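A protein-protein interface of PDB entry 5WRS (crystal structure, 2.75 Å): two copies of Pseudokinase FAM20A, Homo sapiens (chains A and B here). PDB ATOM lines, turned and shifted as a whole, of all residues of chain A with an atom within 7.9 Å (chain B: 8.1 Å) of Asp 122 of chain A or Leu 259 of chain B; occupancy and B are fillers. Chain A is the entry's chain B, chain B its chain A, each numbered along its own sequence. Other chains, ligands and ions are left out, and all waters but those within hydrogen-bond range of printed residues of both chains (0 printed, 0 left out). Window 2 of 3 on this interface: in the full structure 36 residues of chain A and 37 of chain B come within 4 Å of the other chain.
The side-chain sulfur of Cys 123 of chain A sits close to the backbone carbonyl oxygen of Arg 264 of chain B (3.5 Å). The side-chain carboxylate of Glu 327 of chain B lies within hydrogen-bond range of the side-chain hydroxyl of Thr 124 of chain A (2.9 Å). The side-chain hydroxyl (OG) of Ser 266 of chain B lies within hydrogen-bond range of the backbone carbonyl oxygen (O) of Cys 123 of chain A, at 3.3 Å.
The guanidinium group of Arg 264 of chain B lies within salt-bridge range of the side-chain carboxylate of Glu 327 of chain B, at 3.0 Å. The side-chain carboxylate (OD1) of Asp 113 of chain B lies within hydrogen-bond range of the side-chain hydroxyl (OG) of Ser 111 of chain B (2.5 Å). SG of Cys 123 of chain A forms a disulfide with SG of Cys 235 of chain A, 2.1 Å away. SG of Cys 121 of chain A is disulfide-bonded to SG of Cys 231 of chain A (2.1 Å).
Asp 122 of chain A touches Leu 259 of chain B. Thr 124 of chain A touches Ser 266 of chain B. Gln 125 of chain A touches Asp 113 of chain B (OE1 to CB, 3.5 Å). Val 127 of chain A touches Ser 266 of chain B.
Cys 121 of chain A touches none of the printed residues of chain B. Of the printed residues of chain B, Asp 122 of chain A touches Leu 259 (3.9 Å). Printed residues of chain B within 4 Å of Gln 125 of chain A: Asp 113 (3.5 Å). No residue of chain A comes within 4 Å of Ser 258 of chain B. Leu 259 of chain B touches just one residue of chain A: Asp 122 (3.9 Å). Printed residues of chain A within 4 Å of Ser 266 of chain B: Cys 123, Thr 124 and Val 127.
Among the printed residues, 7 pairs touch across the chains. Among the printed residues, no Asp or Glu carboxylate lies within 4 Å of a Lys or Arg side-chain nitrogen of the other chain.
No position is printed for both chains.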
ATOM      1  N   LEU A 117      14.657  16.839   8.187  1.00  0.00           N
ATOM      2  CA  LEU A 117      15.145  17.048   6.827  1.00  0.00           C
ATOM      3  C   LEU A 117      14.116  17.729   5.929  1.00  0.00           C
ATOM      4  O   LEU A 117      14.146  17.558   4.706  1.00  0.00           O
ATOM      5  CB  LEU A 117      15.580  15.717   6.212  1.00  0.00           C
ATOM      6  CG  LEU A 117      16.457  14.833   7.101  1.00  0.00           C
ATOM      7  CD1 LEU A 117      16.830  13.544   6.381  1.00  0.00           C
ATOM      8  CD2 LEU A 117      17.700  15.587   7.551  1.00  0.00           C
ATOM      9  N   GLY A 119      13.674  21.171   5.022  1.00  0.00           N
ATOM     10  CA  GLY A 119      14.439  22.386   5.202  1.00  0.00           C
ATOM     11  C   GLY A 119      14.174  23.488   4.193  1.00  0.00           C
ATOM     12  O   GLY A 119      13.009  23.704   3.851  1.00  0.00           O
ATOM     13  N   ALA A 120      15.197  24.196   3.690  1.00  0.00           N
ATOM     14  CA  ALA A 120      16.646  23.926   3.819  1.00  0.00           C
ATOM     15  C   ALA A 120      17.048  22.543   3.298  1.00  0.00           C
ATOM     16  O   ALA A 120      17.326  21.622   4.068  1.00  0.00           O
ATOM     17  CB  ALA A 120      17.136  24.128   5.271  1.00  0.00           C
ATOM     18  N   CYS A 121      17.076  22.427   1.971  1.00  0.00           N
ATOM     19  CA  CYS A 121      17.353  21.171   1.284  1.00  0.00           C
ATOM     20  C   CYS A 121      18.853  21.045   1.039  1.00  0.00           C
ATOM     21  O   CYS A 121      19.449  21.880   0.350  1.00  0.00           O
ATOM     22  CB  CYS A 121      16.588  21.106  -0.038  1.00  0.00           C
ATOM     23  SG  CYS A 121      16.731  19.538  -0.936  1.00  0.00           S
ATOM     24  N   ASP A 122      19.458  20.004   1.608  1.00  0.00           N
ATOM     25  CA  ASP A 122      20.872  19.703   1.414  1.00  0.00           C
ATOM     26  C   ASP A 122      21.008  18.239   1.029  1.00  0.00           C
ATOM     27  O   ASP A 122      20.592  17.356   1.784  1.00  0.00           O
ATOM     28  CB  ASP A 122      21.679  20.009   2.680  1.00  0.00           C
ATOM     29  CG  ASP A 122      23.124  19.563   2.576  1.00  0.00           C
ATOM     30  OD1 ASP A 122      23.749  19.802   1.522  1.00  0.00           O
ATOM     31  OD2 ASP A 122      23.636  18.971   3.551  1.00  0.00           O
ATOM     32  N   CYS A 123      21.591  17.984  -0.144  1.00  0.00           N
ATOM     33  CA  CYS A 123      21.660  16.631  -0.684  1.00  0.00           C
ATOM     34  C   CYS A 123      22.630  15.730   0.070  1.00  0.00           C
ATOM     35  O   CYS A 123      22.616  14.516  -0.153  1.00  0.00           O
ATOM     36  CB  CYS A 123      22.043  16.680  -2.162  1.00  0.00           C
ATOM     37  SG  CYS A 123      20.865  17.598  -3.171  1.00  0.00           S
ATOM     38  N   THR A 124      23.466  16.284   0.949  1.00  0.00           N
ATOM     39  CA  THR A 124      24.360  15.445   1.740  1.00  0.00           C
ATOM     40  C   THR A 124      23.571  14.564   2.703  1.00  0.00           C
ATOM     41  O   THR A 124      23.833  13.361   2.817  1.00  0.00           O
ATOM     42  CB  THR A 124      25.365  16.316   2.497  1.00  0.00           C
ATOM     43  OG1 THR A 124      26.386  16.757   1.595  1.00  0.00           O
ATOM     44  CG2 THR A 124      26.006  15.536   3.636  1.00  0.00           C
ATOM     45  N   GLN A 125      22.601  15.149   3.406  1.00  0.00           N
ATOM     46  CA  GLN A 125      21.782  14.434   4.381  1.00  0.00           C
ATOM     47  C   GLN A 125      20.587  13.723   3.752  1.00  0.00           C
ATOM     48  O   GLN A 125      19.755  13.176   4.480  1.00  0.00           O
ATOM     49  CB  GLN A 125      21.301  15.405   5.463  1.00  0.00           C
ATOM     50  CG  GLN A 125      20.746  16.706   4.916  1.00  0.00           C
ATOM     51  CD  GLN A 125      20.464  17.727   6.001  1.00  0.00           C
ATOM     52  OE1 GLN A 125      20.892  17.571   7.144  1.00  0.00           O
ATOM     53  NE2 GLN A 125      19.740  18.782   5.646  1.00  0.00           N
ATOM     54  N   ILE A 126      20.489  13.717   2.426  1.00  0.00           N
ATOM     55  CA  ILE A 126      19.384  13.101   1.716  1.00  0.00           C
ATOM     56  C   ILE A 126      19.823  11.844   0.977  1.00  0.00           C
ATOM     57  O   ILE A 126      19.070  10.873   0.906  1.00  0.00           O
ATOM     58  CB  ILE A 126      18.729  14.106   0.742  1.00  0.00           C
ATOM     59  CG1 ILE A 126      18.078  15.250   1.511  1.00  0.00           C
ATOM     60  CG2 ILE A 126      17.703  13.416  -0.160  1.00  0.00           C
ATOM     61  CD1 ILE A 126      16.934  14.810   2.388  1.00  0.00           C
ATOM     62  N   VAL A 127      21.038  11.837   0.434  1.00  0.00           N
ATOM     63  CA  VAL A 127      21.512  10.734  -0.376  1.00  0.00           C
ATOM     64  C   VAL A 127      22.317   9.741   0.473  1.00  0.00           C
ATOM     65  O   VAL A 127      23.094   8.949  -0.057  1.00  0.00           O
ATOM     66  CB  VAL A 127      22.320  11.239  -1.593  1.00  0.00           C
ATOM     67  CG1 VAL A 127      22.594  10.122  -2.588  1.00  0.00           C
ATOM     68  CG2 VAL A 127      21.587  12.375  -2.293  1.00  0.00           C
ATOM     69  N   LYS A 128      22.136   9.771   1.792  1.00  0.00           N
ATOM     70  CA  LYS A 128      22.794   8.806   2.652  1.00  0.00           C
ATOM     71  C   LYS A 128      22.271   7.397   2.378  1.00  0.00           C
ATOM     72  O   LYS A 128      21.111   7.221   2.001  1.00  0.00           O
ATOM     73  CB  LYS A 128      22.586   9.178   4.121  1.00  0.00           C
ATOM     74  CG  LYS A 128      23.461  10.333   4.580  1.00  0.00           C
ATOM     75  CD  LYS A 128      23.313  10.604   6.065  1.00  0.00           C
ATOM     76  CE  LYS A 128      24.007  11.900   6.450  1.00  0.00           C
ATOM     77  NZ  LYS A 128      25.396  11.932   5.918  1.00  0.00           N
ATOM     78  N   HIS A 133      13.575   7.253   2.343  1.00  0.00           N
ATOM     79  CA  HIS A 133      12.696   8.407   2.359  1.00  0.00           C
ATOM     80  C   HIS A 133      11.334   7.988   1.820  1.00  0.00           C
ATOM     81  O   HIS A 133      11.189   6.935   1.192  1.00  0.00           O
ATOM     82  CB  HIS A 133      13.281   9.558   1.542  1.00  0.00           C
ATOM     83  CG  HIS A 133      14.412  10.262   2.224  1.00  0.00           C
ATOM     84  ND1 HIS A 133      14.213  11.253   3.160  1.00  0.00           N
ATOM     85  CD2 HIS A 133      15.753  10.116   2.111  1.00  0.00           C
ATOM     86  CE1 HIS A 133      15.382  11.688   3.594  1.00  0.00           C
ATOM     87  NE2 HIS A 133      16.333  11.015   2.973  1.00  0.00           N
ATOM     88  N   CYS A 231      12.561  17.586  -1.369  1.00  0.00           N
ATOM     89  CA  CYS A 231      14.014  17.681  -1.282  1.00  0.00           C
ATOM     90  C   CYS A 231      14.696  16.513  -1.997  1.00  0.00           C
ATOM     91  O   CYS A 231      15.685  16.735  -2.709  1.00  0.00           O
ATOM     92  CB  CYS A 231      14.454  17.776   0.183  1.00  0.00           C
ATOM     93  SG  CYS A 231      16.223  18.060   0.433  1.00  0.00           S
ATOM     94  N   PRO A 232      14.232  15.266  -1.842  1.00  0.00           N
ATOM     95  CA  PRO A 232      14.787  14.192  -2.686  1.00  0.00           C
ATOM     96  C   PRO A 232      14.587  14.419  -4.175  1.00  0.00           C
ATOM     97  O   PRO A 232      15.430  13.993  -4.974  1.00  0.00           O
ATOM     98  CB  PRO A 232      14.035  12.948  -2.198  1.00  0.00           C
ATOM     99  CG  PRO A 232      13.747  13.242  -0.780  1.00  0.00           C
ATOM    100  CD  PRO A 232      13.413  14.709  -0.749  1.00  0.00           C
ATOM    101  N   CYS A 235      17.326  16.644  -5.397  1.00  0.00           N
ATOM    102  CA  CYS A 235      18.591  15.923  -5.392  1.00  0.00           C
ATOM    103  C   CYS A 235      18.620  14.777  -6.395  1.00  0.00           C
ATOM    104  O   CYS A 235      19.619  14.048  -6.447  1.00  0.00           O
ATOM    105  CB  CYS A 235      18.890  15.399  -3.987  1.00  0.00           C
ATOM    106  SG  CYS A 235      19.045  16.713  -2.757  1.00  0.00           S
ATOM    107  N   LEU B  29      30.147  31.160 -10.362  1.00  0.00           N
ATOM    108  CA  LEU B  29      29.227  32.229 -10.008  1.00  0.00           C
ATOM    109  C   LEU B  29      29.226  33.320 -11.069  1.00  0.00           C
ATOM    110  O   LEU B  29      30.238  33.576 -11.728  1.00  0.00           O
ATOM    111  CB  LEU B  29      29.597  32.843  -8.656  1.00  0.00           C
ATOM    112  CG  LEU B  29      29.683  31.913  -7.447  1.00  0.00           C
ATOM    113  CD1 LEU B  29      30.038  32.704  -6.199  1.00  0.00           C
ATOM    114  CD2 LEU B  29      28.376  31.166  -7.258  1.00  0.00           C
ATOM    115  N   TYR B  37      23.707  39.313  -3.961  1.00  0.00           N
ATOM    116  CA  TYR B  37      23.220  38.345  -2.986  1.00  0.00           C
ATOM    117  C   TYR B  37      24.000  38.441  -1.681  1.00  0.00           C
ATOM    118  O   TYR B  37      23.413  38.392  -0.595  1.00  0.00           O
ATOM    119  CB  TYR B  37      23.307  36.935  -3.572  1.00  0.00           C
ATOM    120  CG  TYR B  37      22.928  35.830  -2.611  1.00  0.00           C
ATOM    121  CD1 TYR B  37      21.598  35.478  -2.417  1.00  0.00           C
ATOM    122  CD2 TYR B  37      23.900  35.126  -1.910  1.00  0.00           C
ATOM    123  CE1 TYR B  37      21.247  34.466  -1.544  1.00  0.00           C
ATOM    124  CE2 TYR B  37      23.559  34.114  -1.036  1.00  0.00           C
ATOM    125  CZ  TYR B  37      22.231  33.788  -0.857  1.00  0.00           C
ATOM    126  OH  TYR B  37      21.884  32.780   0.011  1.00  0.00           O
ATOM    127  N   TYR B  38      25.325  38.573  -1.770  1.00  0.00           N
ATOM    128  CA  TYR B  38      26.133  38.733  -0.567  1.00  0.00           C
ATOM    129  C   TYR B  38      25.879  40.075   0.109  1.00  0.00           C
ATOM    130  O   TYR B  38      25.936  40.166   1.340  1.00  0.00           O
ATOM    131  CB  TYR B  38      27.615  38.569  -0.903  1.00  0.00           C
ATOM    132  CG  TYR B  38      28.017  37.145  -1.226  1.00  0.00           C
ATOM    133  CD1 TYR B  38      27.377  36.070  -0.622  1.00  0.00           C
ATOM    134  CD2 TYR B  38      29.036  36.876  -2.130  1.00  0.00           C
ATOM    135  CE1 TYR B  38      27.741  34.767  -0.911  1.00  0.00           C
ATOM    136  CE2 TYR B  38      29.406  35.575  -2.426  1.00  0.00           C
ATOM    137  CZ  TYR B  38      28.755  34.526  -1.811  1.00  0.00           C
ATOM    138  OH  TYR B  38      29.117  33.230  -2.100  1.00  0.00           O
ATOM    139  N   SER B 111      26.297  24.038  13.018  1.00  0.00           N
ATOM    140  CA  SER B 111      26.092  23.675  11.626  1.00  0.00           C
ATOM    141  C   SER B 111      24.607  23.443  11.373  1.00  0.00           C
ATOM    142  O   SER B 111      23.858  23.037  12.265  1.00  0.00           O
ATOM    143  CB  SER B 111      26.894  22.422  11.278  1.00  0.00           C
ATOM    144  OG  SER B 111      26.552  21.936   9.992  1.00  0.00           O
ATOM    145  N   GLN B 112      24.178  23.722  10.139  1.00  0.00           N
ATOM    146  CA  GLN B 112      22.755  23.645   9.824  1.00  0.00           C
ATOM    147  C   GLN B 112      22.224  22.224   9.976  1.00  0.00           C
ATOM    148  O   GLN B 112      21.086  22.023  10.417  1.00  0.00           O
ATOM    149  CB  GLN B 112      22.502  24.164   8.409  1.00  0.00           C
ATOM    150  CG  GLN B 112      21.043  24.475   8.120  1.00  0.00           C
ATOM    151  CD  GLN B 112      20.521  25.635   8.948  1.00  0.00           C
ATOM    152  OE1 GLN B 112      21.248  26.585   9.236  1.00  0.00           O
ATOM    153  NE2 GLN B 112      19.252  25.558   9.340  1.00  0.00           N
ATOM    154  N   ASP B 113      23.032  21.222   9.617  1.00  0.00           N
ATOM    155  CA  ASP B 113      22.587  19.835   9.720  1.00  0.00           C
ATOM    156  C   ASP B 113      22.492  19.358  11.162  1.00  0.00           C
ATOM    157  O   ASP B 113      21.860  18.328  11.421  1.00  0.00           O
ATOM    158  CB  ASP B 113      23.524  18.915   8.935  1.00  0.00           C
ATOM    159  CG  ASP B 113      24.934  18.894   9.497  1.00  0.00           C
ATOM    160  OD1 ASP B 113      25.290  19.816  10.261  1.00  0.00           O
ATOM    161  OD2 ASP B 113      25.685  17.949   9.180  1.00  0.00           O
ATOM    162  N   LEU B 256      32.218  26.892   0.962  1.00  0.00           N
ATOM    163  CA  LEU B 256      31.882  27.007  -0.443  1.00  0.00           C
ATOM    164  C   LEU B 256      30.758  28.029  -0.601  1.00  0.00           C
ATOM    165  O   LEU B 256      30.139  28.441   0.384  1.00  0.00           O
ATOM    166  CB  LEU B 256      31.481  25.639  -0.993  1.00  0.00           C
ATOM    167  CG  LEU B 256      32.563  24.559  -0.951  1.00  0.00           C
ATOM    168  CD1 LEU B 256      32.037  23.245  -1.508  1.00  0.00           C
ATOM    169  CD2 LEU B 256      33.808  25.009  -1.701  1.00  0.00           C
ATOM    170  N   PRO B 257      30.478  28.474  -1.826  1.00  0.00           N
ATOM    171  CA  PRO B 257      29.368  29.415  -2.016  1.00  0.00           C
ATOM    172  C   PRO B 257      28.041  28.794  -1.612  1.00  0.00           C
ATOM    173  O   PRO B 257      27.873  27.573  -1.617  1.00  0.00           O
ATOM    174  CB  PRO B 257      29.415  29.730  -3.517  1.00  0.00           C
ATOM    175  CG  PRO B 257      30.239  28.641  -4.120  1.00  0.00           C
ATOM    176  CD  PRO B 257      31.236  28.278  -3.073  1.00  0.00           C
ATOM    177  N   SER B 258      27.100  29.661  -1.242  1.00  0.00           N
ATOM    178  CA  SER B 258      25.774  29.221  -0.827  1.00  0.00           C
ATOM    179  C   SER B 258      25.135  28.322  -1.878  1.00  0.00           C
ATOM    180  O   SER B 258      25.325  28.514  -3.083  1.00  0.00           O
ATOM    181  CB  SER B 258      24.878  30.434  -0.571  1.00  0.00           C
ATOM    182  OG  SER B 258      23.644  30.039  -0.003  1.00  0.00           O
ATOM    183  N   LEU B 259      24.372  27.331  -1.407  1.00  0.00           N
ATOM    184  CA  LEU B 259      23.635  26.464  -2.316  1.00  0.00           C
ATOM    185  C   LEU B 259      22.588  27.234  -3.109  1.00  0.00           C
ATOM    186  O   LEU B 259      22.161  26.764  -4.169  1.00  0.00           O
ATOM    187  CB  LEU B 259      22.979  25.322  -1.539  1.00  0.00           C
ATOM    188  CG  LEU B 259      23.950  24.367  -0.844  1.00  0.00           C
ATOM    189  CD1 LEU B 259      23.199  23.396   0.047  1.00  0.00           C
ATOM    190  CD2 LEU B 259      24.784  23.621  -1.871  1.00  0.00           C
ATOM    191  N   ASN B 260      22.166  28.401  -2.618  1.00  0.00           N
ATOM    192  CA  ASN B 260      21.296  29.265  -3.410  1.00  0.00           C
ATOM    193  C   ASN B 260      22.017  29.772  -4.653  1.00  0.00           C
ATOM    194  O   ASN B 260      21.403  29.939  -5.714  1.00  0.00           O
ATOM    195  CB  ASN B 260      20.807  30.439  -2.562  1.00  0.00           C
ATOM    196  CG  ASN B 260      20.002  29.995  -1.356  1.00  0.00           C
ATOM    197  OD1 ASN B 260      19.133  29.129  -1.459  1.00  0.00           O
ATOM    198  ND2 ASN B 260      20.288  30.588  -0.201  1.00  0.00           N
ATOM    199  N   LEU B 261      23.319  30.035  -4.538  1.00  0.00           N
ATOM    200  CA  LEU B 261      24.115  30.497  -5.668  1.00  0.00           C
ATOM    201  C   LEU B 261      24.660  29.349  -6.511  1.00  0.00           C
ATOM    202  O   LEU B 261      24.756  29.475  -7.736  1.00  0.00           O
ATOM    203  CB  LEU B 261      25.279  31.361  -5.175  1.00  0.00           C
ATOM    204  CG  LEU B 261      24.926  32.704  -4.537  1.00  0.00           C
ATOM    205  CD1 LEU B 261      26.190  33.403  -4.064  1.00  0.00           C
ATOM    206  CD2 LEU B 261      24.154  33.578  -5.511  1.00  0.00           C
ATOM    207  N   ALA B 262      25.016  28.229  -5.882  1.00  0.00           N
ATOM    208  CA  ALA B 262      25.630  27.104  -6.585  1.00  0.00           C
ATOM    209  C   ALA B 262      25.119  25.798  -5.997  1.00  0.00           C
ATOM    210  O   ALA B 262      25.676  25.279  -5.021  1.00  0.00           O
ATOM    211  CB  ALA B 262      27.156  27.172  -6.513  1.00  0.00           C
ATOM    212  N   PRO B 263      24.059  25.233  -6.571  1.00  0.00           N
ATOM    213  CA  PRO B 263      23.535  23.965  -6.054  1.00  0.00           C
ATOM    214  C   PRO B 263      24.510  22.825  -6.292  1.00  0.00           C
ATOM    215  O   PRO B 263      25.270  22.811  -7.262  1.00  0.00           O
ATOM    216  CB  PRO B 263      22.238  23.761  -6.847  1.00  0.00           C
ATOM    217  CG  PRO B 263      21.934  25.088  -7.477  1.00  0.00           C
ATOM    218  CD  PRO B 263      23.250  25.762  -7.679  1.00  0.00           C
ATOM    219  N   ARG B 264      24.477  21.856  -5.383  1.00  0.00           N
ATOM    220  CA  ARG B 264      25.359  20.703  -5.433  1.00  0.00           C
ATOM    221  C   ARG B 264      24.552  19.417  -5.342  1.00  0.00           C
ATOM    222  O   ARG B 264      23.487  19.372  -4.719  1.00  0.00           O
ATOM    223  CB  ARG B 264      26.393  20.761  -4.308  1.00  0.00           C
ATOM    224  CG  ARG B 264      27.421  21.861  -4.484  1.00  0.00           C
ATOM    225  CD  ARG B 264      28.426  21.825  -3.359  1.00  0.00           C
ATOM    226  NE  ARG B 264      27.809  22.311  -2.130  1.00  0.00           N
ATOM    227  CZ  ARG B 264      28.258  22.052  -0.909  1.00  0.00           C
ATOM    228  NH1 ARG B 264      29.333  21.299  -0.748  1.00  0.00           N
ATOM    229  NH2 ARG B 264      27.631  22.542   0.149  1.00  0.00           N
ATOM    230  N   LEU B 265      25.074  18.373  -5.978  1.00  0.00           N
ATOM    231  CA  LEU B 265      24.501  17.039  -5.929  1.00  0.00           C
ATOM    232  C   LEU B 265      25.430  16.099  -5.171  1.00  0.00           C
ATOM    233  O   LEU B 265      26.653  16.229  -5.237  1.00  0.00           O
ATOM    234  CB  LEU B 265      24.262  16.495  -7.341  1.00  0.00           C
ATOM    235  CG  LEU B 265      23.250  17.242  -8.210  1.00  0.00           C
ATOM    236  CD1 LEU B 265      23.192  16.627  -9.600  1.00  0.00           C
ATOM    237  CD2 LEU B 265      21.876  17.244  -7.562  1.00  0.00           C
ATOM    238  N   SER B 266      24.838  15.152  -4.451  1.00  0.00           N
ATOM    239  CA  SER B 266      25.582  14.071  -3.819  1.00  0.00           C
ATOM    240  C   SER B 266      25.379  12.798  -4.629  1.00  0.00           C
ATOM    241  O   SER B 266      24.243  12.450  -4.970  1.00  0.00           O
ATOM    242  CB  SER B 266      25.132  13.856  -2.373  1.00  0.00           C
ATOM    243  OG  SER B 266      25.561  14.918  -1.540  1.00  0.00           O
ATOM    244  N   GLU B 327      30.551  14.952  -4.242  1.00  0.00           N
ATOM    245  CA  GLU B 327      29.690  16.075  -4.575  1.00  0.00           C
ATOM    246  C   GLU B 327      30.178  16.775  -5.837  1.00  0.00           C
ATOM    247  O   GLU B 327      31.372  16.772  -6.149  1.00  0.00           O
ATOM    248  CB  GLU B 327      29.609  17.072  -3.414  1.00  0.00           C
ATOM    249  CG  GLU B 327      28.943  16.495  -2.173  1.00  0.00           C
ATOM    250  CD  GLU B 327      28.629  17.550  -1.131  1.00  0.00           C
ATOM    251  OE1 GLU B 327      28.234  18.670  -1.518  1.00  0.00           O
ATOM    252  OE2 GLU B 327      28.773  17.258   0.075  1.00  0.00           O
ATOM    253  N   MET B 328      29.233  17.377  -6.558  1.00  0.00           N
ATOM    254  CA  MET B 328      29.509  18.090  -7.796  1.00  0.00           C
ATOM    255  C   MET B 328      28.677  19.362  -7.833  1.00  0.00           C
ATOM    256  O   MET B 328      27.623  19.454  -7.200  1.00  0.00           O
ATOM    257  CB  MET B 328      29.183  17.249  -9.039  1.00  0.00           C
ATOM    258  CG  MET B 328      29.792  15.866  -9.077  1.00  0.00           C
ATOM    259  SD  MET B 328      29.335  15.023 -10.603  1.00  0.00           S
ATOM    260  CE  MET B 328      30.134  16.065 -11.822  1.00  0.00           C
ATOM    261  N   PHE B 329      29.153  20.343  -8.596  1.00  0.00           N
ATOM    262  CA  PHE B 329      28.374  21.548  -8.845  1.00  0.00           C
ATOM    263  C   PHE B 329      27.393  21.304  -9.985  1.00  0.00           C
ATOM    264  O   PHE B 329      27.755  20.726 -11.016  1.00  0.00           O
ATOM    265  CB  PHE B 329      29.289  22.728  -9.169  1.00  0.00           C
ATOM    266  CG  PHE B 329      30.101  23.207  -7.999  1.00  0.00           C
ATOM    267  CD1 PHE B 329      29.484  23.784  -6.901  1.00  0.00           C
ATOM    268  CD2 PHE B 329      31.482  23.096  -8.002  1.00  0.00           C
ATOM    269  CE1 PHE B 329      30.228  24.230  -5.822  1.00  0.00           C
ATOM    270  CE2 PHE B 329      32.232  23.544  -6.930  1.00  0.00           C
ATOM    271  CZ  PHE B 329      31.604  24.110  -5.838  1.00  0.00           C
ATOM    272  N   THR B 330      26.145  21.742  -9.791  1.00  0.00           N
ATOM    273  CA  THR B 330      25.111  21.542 -10.802  1.00  0.00           C
ATOM    274  C   THR B 330      25.456  22.255 -12.104  1.00  0.00           C
ATOM    275  O   THR B 330      25.197  21.731 -13.194  1.00  0.00           O
ATOM    276  CB  THR B 330      23.759  22.016 -10.263  1.00  0.00           C
ATOM    277  OG1 THR B 330      23.299  21.104  -9.260  1.00  0.00           O
ATOM    278  CG2 THR B 330      22.721  22.090 -11.375  1.00  0.00           C
ATOM    279  N   LEU B 341      35.180  16.721  -0.322  1.00  0.00           N
ATOM    280  CA  LEU B 341      34.808  17.321   0.948  1.00  0.00           C
ATOM    281  C   LEU B 341      35.031  16.359   2.111  1.00  0.00           C
ATOM    282  O   LEU B 341      35.079  15.140   1.943  1.00  0.00           O
ATOM    283  CB  LEU B 341      33.339  17.734   0.921  1.00  0.00           C
ATOM    284  CG  LEU B 341      32.983  19.215   0.972  1.00  0.00           C
ATOM    285  CD1 LEU B 341      34.052  20.031   0.299  1.00  0.00           C
ATOM    286  CD2 LEU B 341      31.654  19.423   0.288  1.00  0.00           C
